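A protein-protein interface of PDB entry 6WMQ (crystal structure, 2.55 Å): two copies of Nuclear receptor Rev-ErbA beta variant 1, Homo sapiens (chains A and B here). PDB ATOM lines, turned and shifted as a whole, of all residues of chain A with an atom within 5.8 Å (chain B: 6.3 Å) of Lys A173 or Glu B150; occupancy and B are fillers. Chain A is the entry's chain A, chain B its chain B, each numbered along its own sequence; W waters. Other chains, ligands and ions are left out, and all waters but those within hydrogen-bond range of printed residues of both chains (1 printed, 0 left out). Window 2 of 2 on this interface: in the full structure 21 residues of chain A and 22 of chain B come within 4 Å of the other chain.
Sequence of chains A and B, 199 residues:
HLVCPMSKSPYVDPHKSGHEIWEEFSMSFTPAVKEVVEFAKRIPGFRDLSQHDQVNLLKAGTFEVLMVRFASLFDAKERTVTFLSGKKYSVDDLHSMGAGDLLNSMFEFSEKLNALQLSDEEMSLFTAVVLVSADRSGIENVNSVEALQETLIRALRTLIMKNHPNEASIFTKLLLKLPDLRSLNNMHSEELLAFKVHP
No position is printed for both chains.
Of the 4 pairs that touch across the chains among the printed residues, none has its exchanged pair printed and touching as well.
Lys A173 touches one residue of chain B.
Of the printed residues of chain A, Glu B146 touches Lys A112.
Of the printed residues of chain A, Ile B153 touches Thr A172.
The nearest residue of chain B that does not touch Lys A173 is Glu B146 (5.2 Å).
The nearest printed residue of chain B that does not touch Lys A112 is Ala B147 (8.3 Å).
OE2 of Glu B146 is in salt-bridge range of NZ of Lys A112, 2.9 Å away.
Among the printed residues, merely in contact across the chains: Thr A172 with Ile B153 (3.6 Å), Lys A173 with Glu B150 (3.8 Å) and Leu A176 with Gln B149 (3.96 Å).
Of the 11 printed residues of chain A, 4 touch a printed residue of chain B.
Hydrophobic or aromatic side chains of chain A that line the printed part of chain B: Leu A176.
Among the printed residues, 4 pairs touch across the chains.
Among the printed residues, Asp or Glu carboxylates within 4 Å of a Lys or Arg side-chain nitrogen of the other chain: Lys A112 with Glu B146.
Water W1 lies within hydrogen-bond range of O of Leu A176 (2.8 Å) and NE2 of Gln B149 (3.3 Å).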
ATOM      1  N   LYS A 112     -17.339  -5.508  31.503  1.00  0.00           N
ATOM      2  CA  LYS A 112     -17.291  -4.119  31.057  1.00  0.00           C
ATOM      3  C   LYS A 112     -17.792  -3.962  29.623  1.00  0.00           C
ATOM      4  O   LYS A 112     -18.445  -2.963  29.299  1.00  0.00           O
ATOM      5  CB  LYS A 112     -15.873  -3.581  31.188  1.00  0.00           C
ATOM      6  CG  LYS A 112     -15.422  -3.476  32.615  1.00  0.00           C
ATOM      7  CD  LYS A 112     -16.141  -2.355  33.323  1.00  0.00           C
ATOM      8  CE  LYS A 112     -15.417  -1.995  34.603  1.00  0.00           C
ATOM      9  NZ  LYS A 112     -13.965  -2.233  34.443  1.00  0.00           N
ATOM     10  N   LEU A 116     -21.629  -2.298  27.855  1.00  0.00           N
ATOM     11  CA  LEU A 116     -21.903  -1.285  26.837  1.00  0.00           C
ATOM     12  C   LEU A 116     -23.106  -1.662  25.985  1.00  0.00           C
ATOM     13  O   LEU A 116     -23.711  -0.784  25.361  1.00  0.00           O
ATOM     14  CB  LEU A 116     -20.677  -1.079  25.951  1.00  0.00           C
ATOM     15  CG  LEU A 116     -19.474  -0.362  26.560  1.00  0.00           C
ATOM     16  CD1 LEU A 116     -18.225  -0.729  25.796  1.00  0.00           C
ATOM     17  CD2 LEU A 116     -19.665   1.141  26.562  1.00  0.00           C
ATOM     18  N   SER A 169     -18.508   9.424  24.873  1.00  0.00           N
ATOM     19  CA  SER A 169     -17.415   8.730  25.533  1.00  0.00           C
ATOM     20  C   SER A 169     -17.388   7.223  25.270  1.00  0.00           C
ATOM     21  O   SER A 169     -16.354   6.593  25.530  1.00  0.00           O
ATOM     22  CB  SER A 169     -17.482   8.993  27.034  1.00  0.00           C
ATOM     23  OG  SER A 169     -18.485   8.204  27.655  1.00  0.00           O
ATOM     24  N   ILE A 170     -18.479   6.623  24.779  1.00  0.00           N
ATOM     25  CA  ILE A 170     -18.439   5.204  24.421  1.00  0.00           C
ATOM     26  C   ILE A 170     -17.316   4.943  23.425  1.00  0.00           C
ATOM     27  O   ILE A 170     -16.621   3.919  23.497  1.00  0.00           O
ATOM     28  CB  ILE A 170     -19.795   4.747  23.860  1.00  0.00           C
ATOM     29  CG1 ILE A 170     -20.873   4.856  24.926  1.00  0.00           C
ATOM     30  CG2 ILE A 170     -19.724   3.316  23.362  1.00  0.00           C
ATOM     31  CD1 ILE A 170     -22.252   4.483  24.435  1.00  0.00           C
ATOM     32  N   PHE A 171     -17.108   5.878  22.495  1.00  0.00           N
ATOM     33  CA  PHE A 171     -16.113   5.674  21.453  1.00  0.00           C
ATOM     34  C   PHE A 171     -14.716   5.530  22.045  1.00  0.00           C
ATOM     35  O   PHE A 171     -13.996   4.581  21.729  1.00  0.00           O
ATOM     36  CB  PHE A 171     -16.172   6.820  20.452  1.00  0.00           C
ATOM     37  CG  PHE A 171     -15.084   6.781  19.447  1.00  0.00           C
ATOM     38  CD1 PHE A 171     -15.053   5.780  18.480  1.00  0.00           C
ATOM     39  CD2 PHE A 171     -14.074   7.729  19.468  1.00  0.00           C
ATOM     40  CE1 PHE A 171     -14.038   5.743  17.545  1.00  0.00           C
ATOM     41  CE2 PHE A 171     -13.053   7.697  18.527  1.00  0.00           C
ATOM     42  CZ  PHE A 171     -13.037   6.707  17.574  1.00  0.00           C
ATOM     43  N   THR A 172     -14.318   6.464  22.907  1.00  0.00           N
ATOM     44  CA  THR A 172     -13.014   6.364  23.564  1.00  0.00           C
ATOM     45  C   THR A 172     -12.926   5.125  24.455  1.00  0.00           C
ATOM     46  O   THR A 172     -11.883   4.461  24.500  1.00  0.00           O
ATOM     47  CB  THR A 172     -12.737   7.627  24.379  1.00  0.00           C
ATOM     48  OG1 THR A 172     -13.113   8.778  23.613  1.00  0.00           O
ATOM     49  CG2 THR A 172     -11.261   7.725  24.721  1.00  0.00           C
ATOM     50  N   LYS A 173     -14.015   4.792  25.155  1.00  0.00           N
ATOM     51  CA  LYS A 173     -14.044   3.572  25.954  1.00  0.00           C
ATOM     52  C   LYS A 173     -13.791   2.341  25.092  1.00  0.00           C
ATOM     53  O   LYS A 173     -13.098   1.408  25.520  1.00  0.00           O
ATOM     54  CB  LYS A 173     -15.377   3.447  26.693  1.00  0.00           C
ATOM     55  CG  LYS A 173     -15.275   3.833  28.168  1.00  0.00           C
ATOM     56  CD  LYS A 173     -16.383   3.219  29.020  1.00  0.00           C
ATOM     57  CE  LYS A 173     -15.821   2.633  30.326  1.00  0.00           C
ATOM     58  NZ  LYS A 173     -16.784   1.743  31.045  1.00  0.00           N
ATOM     59  N   LEU A 174     -14.316   2.331  23.864  1.00  0.00           N
ATOM     60  CA  LEU A 174     -14.071   1.217  22.953  1.00  0.00           C
ATOM     61  C   LEU A 174     -12.613   1.168  22.498  1.00  0.00           C
ATOM     62  O   LEU A 174     -12.055   0.081  22.321  1.00  0.00           O
ATOM     63  CB  LEU A 174     -15.001   1.308  21.750  1.00  0.00           C
ATOM     64  CG  LEU A 174     -16.454   0.926  22.013  1.00  0.00           C
ATOM     65  CD1 LEU A 174     -17.310   1.235  20.789  1.00  0.00           C
ATOM     66  CD2 LEU A 174     -16.558  -0.550  22.398  1.00  0.00           C
ATOM     67  N   LEU A 175     -11.976   2.326  22.299  1.00  0.00           N
ATOM     68  CA  LEU A 175     -10.571   2.299  21.897  1.00  0.00           C
ATOM     69  C   LEU A 175      -9.697   1.780  23.027  1.00  0.00           C
ATOM     70  O   LEU A 175      -8.777   0.987  22.802  1.00  0.00           O
ATOM     71  CB  LEU A 175     -10.102   3.684  21.472  1.00  0.00           C
ATOM     72  CG  LEU A 175     -10.653   4.226  20.150  1.00  0.00           C
ATOM     73  CD1 LEU A 175      -9.832   5.435  19.684  1.00  0.00           C
ATOM     74  CD2 LEU A 175     -10.686   3.151  19.081  1.00  0.00           C
ATOM     75  N   LEU A 176      -9.993   2.198  24.255  1.00  0.00           N
ATOM     76  CA  LEU A 176      -9.193   1.813  25.399  1.00  0.00           C
ATOM     77  C   LEU A 176      -9.333   0.336  25.727  1.00  0.00           C
ATOM     78  O   LEU A 176      -8.576  -0.178  26.545  1.00  0.00           O
ATOM     79  CB  LEU A 176      -9.576   2.687  26.589  1.00  0.00           C
ATOM     80  CG  LEU A 176      -9.248   4.164  26.368  1.00  0.00           C
ATOM     81  CD1 LEU A 176      -9.795   4.989  27.520  1.00  0.00           C
ATOM     82  CD2 LEU A 176      -7.747   4.379  26.205  1.00  0.00           C
ATOM     83  N   LYS A 177     -10.259  -0.363  25.086  1.00  0.00           N
ATOM     84  CA  LYS A 177     -10.264  -1.807  25.176  1.00  0.00           C
ATOM     85  C   LYS A 177      -9.154  -2.446  24.347  1.00  0.00           C
ATOM     86  O   LYS A 177      -8.761  -3.577  24.650  1.00  0.00           O
ATOM     87  CB  LYS A 177     -11.631  -2.335  24.752  1.00  0.00           C
ATOM     88  CG  LYS A 177     -12.661  -2.160  25.854  1.00  0.00           C
ATOM     89  CD  LYS A 177     -14.072  -2.411  25.376  1.00  0.00           C
ATOM     90  CE  LYS A 177     -14.954  -2.854  26.530  1.00  0.00           C
ATOM     91  NZ  LYS A 177     -15.126  -1.830  27.613  1.00  0.00           N
ATOM     92  N   VAL B 145      -8.918   3.189  38.753  1.00  0.00           N
ATOM     93  CA  VAL B 145      -7.864   3.318  37.746  1.00  0.00           C
ATOM     94  C   VAL B 145      -8.443   3.772  36.417  1.00  0.00           C
ATOM     95  O   VAL B 145      -7.863   4.619  35.724  1.00  0.00           O
ATOM     96  CB  VAL B 145      -7.111   1.990  37.583  1.00  0.00           C
ATOM     97  CG1 VAL B 145      -5.983   2.142  36.546  1.00  0.00           C
ATOM     98  CG2 VAL B 145      -6.601   1.530  38.924  1.00  0.00           C
ATOM     99  N   GLU B 146      -9.584   3.204  36.027  1.00  0.00           N
ATOM    100  CA  GLU B 146     -10.171   3.541  34.741  1.00  0.00           C
ATOM    101  C   GLU B 146     -10.833   4.906  34.758  1.00  0.00           C
ATOM    102  O   GLU B 146     -10.963   5.526  33.697  1.00  0.00           O
ATOM    103  CB  GLU B 146     -11.147   2.446  34.318  1.00  0.00           C
ATOM    104  CG  GLU B 146     -10.406   1.275  33.682  1.00  0.00           C
ATOM    105  CD  GLU B 146     -11.278   0.067  33.415  1.00  0.00           C
ATOM    106  OE1 GLU B 146     -10.721  -0.991  33.019  1.00  0.00           O
ATOM    107  OE2 GLU B 146     -12.510   0.175  33.617  1.00  0.00           O
ATOM    108  N   ALA B 147     -11.201   5.402  35.940  1.00  0.00           N
ATOM    109  CA  ALA B 147     -11.692   6.768  36.058  1.00  0.00           C
ATOM    110  C   ALA B 147     -10.549   7.771  35.951  1.00  0.00           C
ATOM    111  O   ALA B 147     -10.707   8.844  35.349  1.00  0.00           O
ATOM    112  CB  ALA B 147     -12.433   6.944  37.386  1.00  0.00           C
ATOM    113  N   LEU B 148      -9.401   7.446  36.547  1.00  0.00           N
ATOM    114  CA  LEU B 148      -8.212   8.267  36.366  1.00  0.00           C
ATOM    115  C   LEU B 148      -7.769   8.260  34.911  1.00  0.00           C
ATOM    116  O   LEU B 148      -7.403   9.301  34.359  1.00  0.00           O
ATOM    117  CB  LEU B 148      -7.089   7.763  37.266  1.00  0.00           C
ATOM    118  CG  LEU B 148      -5.894   8.693  37.326  1.00  0.00           C
ATOM    119  CD1 LEU B 148      -6.359  10.117  37.621  1.00  0.00           C
ATOM    120  CD2 LEU B 148      -4.896   8.202  38.360  1.00  0.00           C
ATOM    121  N   GLN B 149      -7.803   7.093  34.274  1.00  0.00           N
ATOM    122  CA  GLN B 149      -7.403   7.005  32.878  1.00  0.00           C
ATOM    123  C   GLN B 149      -8.345   7.808  31.992  1.00  0.00           C
ATOM    124  O   GLN B 149      -7.902   8.622  31.174  1.00  0.00           O
ATOM    125  CB  GLN B 149      -7.349   5.538  32.456  1.00  0.00           C
ATOM    126  CG  GLN B 149      -7.249   5.307  30.967  1.00  0.00           C
ATOM    127  CD  GLN B 149      -7.531   3.864  30.604  1.00  0.00           C
ATOM    128  OE1 GLN B 149      -8.548   3.294  31.016  1.00  0.00           O
ATOM    129  NE2 GLN B 149      -6.624   3.254  29.835  1.00  0.00           N
ATOM    130  N   GLU B 150      -9.657   7.615  32.170  1.00  0.00           N
ATOM    131  CA  GLU B 150     -10.639   8.338  31.367  1.00  0.00           C
ATOM    132  C   GLU B 150     -10.503   9.854  31.529  1.00  0.00           C
ATOM    133  O   GLU B 150     -10.709  10.598  30.564  1.00  0.00           O
ATOM    134  CB  GLU B 150     -12.051   7.875  31.733  1.00  0.00           C
ATOM    135  CG  GLU B 150     -12.873   7.222  30.624  1.00  0.00           C
ATOM    136  CD  GLU B 150     -14.368   7.122  30.978  1.00  0.00           C
ATOM    137  OE1 GLU B 150     -15.145   8.058  30.661  1.00  0.00           O
ATOM    138  OE2 GLU B 150     -14.765   6.101  31.587  1.00  0.00           O
ATOM    139  N   THR B 151     -10.129  10.337  32.712  1.00  0.00           N
ATOM    140  CA  THR B 151     -10.014  11.788  32.867  1.00  0.00           C
ATOM    141  C   THR B 151      -8.712  12.308  32.268  1.00  0.00           C
ATOM    142  O   THR B 151      -8.683  13.404  31.690  1.00  0.00           O
ATOM    143  CB  THR B 151     -10.094  12.201  34.340  1.00  0.00           C
ATOM    144  OG1 THR B 151     -10.996  11.343  35.031  1.00  0.00           O
ATOM    145  CG2 THR B 151     -10.688  13.599  34.419  1.00  0.00           C
ATOM    146  N   LEU B 152      -7.619  11.553  32.419  1.00  0.00           N
ATOM    147  CA  LEU B 152      -6.383  11.923  31.741  1.00  0.00           C
ATOM    148  C   LEU B 152      -6.586  11.936  30.233  1.00  0.00           C
ATOM    149  O   LEU B 152      -6.235  12.910  29.557  1.00  0.00           O
ATOM    150  CB  LEU B 152      -5.261  10.972  32.155  1.00  0.00           C
ATOM    151  CG  LEU B 152      -4.944  11.167  33.629  1.00  0.00           C
ATOM    152  CD1 LEU B 152      -3.839  10.239  34.064  1.00  0.00           C
ATOM    153  CD2 LEU B 152      -4.569  12.623  33.859  1.00  0.00           C
ATOM    154  N   ILE B 153      -7.208  10.882  29.699  1.00  0.00           N
ATOM    155  CA  ILE B 153      -7.497  10.818  28.268  1.00  0.00           C
ATOM    156  C   ILE B 153      -8.278  12.043  27.817  1.00  0.00           C
ATOM    157  O   ILE B 153      -8.001  12.625  26.758  1.00  0.00           O
ATOM    158  CB  ILE B 153      -8.257   9.530  27.935  1.00  0.00           C
ATOM    159  CG1 ILE B 153      -7.280   8.387  27.934  1.00  0.00           C
ATOM    160  CG2 ILE B 153      -8.908   9.653  26.571  1.00  0.00           C
ATOM    161  CD1 ILE B 153      -6.320   8.605  26.864  1.00  0.00           C
ATOM    162  N   ARG B 154      -9.274  12.445  28.613  1.00  0.00           N
ATOM    163  CA  ARG B 154     -10.093  13.592  28.238  1.00  0.00           C
ATOM    164  C   ARG B 154      -9.274  14.869  28.292  1.00  0.00           C
ATOM    165  O   ARG B 154      -9.346  15.698  27.375  1.00  0.00           O
ATOM    166  CB  ARG B 154     -11.323  13.694  29.138  1.00  0.00           C
ATOM    167  CG  ARG B 154     -12.387  14.645  28.582  1.00  0.00           C
ATOM    168  CD  ARG B 154     -13.549  14.891  29.550  1.00  0.00           C
ATOM    169  NE  ARG B 154     -13.130  15.085  30.937  1.00  0.00           N
ATOM    170  CZ  ARG B 154     -13.848  14.694  31.981  1.00  0.00           C
ATOM    171  NH1 ARG B 154     -15.004  14.095  31.781  1.00  0.00           N
ATOM    172  NH2 ARG B 154     -13.425  14.904  33.217  1.00  0.00           N
ATOM    173  N   ALA B 155      -8.472  15.029  29.347  1.00  0.00           N
ATOM    174  CA  ALA B 155      -7.574  16.172  29.410  1.00  0.00           C
ATOM    175  C   ALA B 155      -6.667  16.200  28.195  1.00  0.00           C
ATOM    176  O   ALA B 155      -6.433  17.265  27.607  1.00  0.00           O
ATOM    177  CB  ALA B 155      -6.746  16.125  30.684  1.00  0.00           C
HETATM  178  O   HOH W   1      -6.896   0.092  28.785  1.00  0.00           O
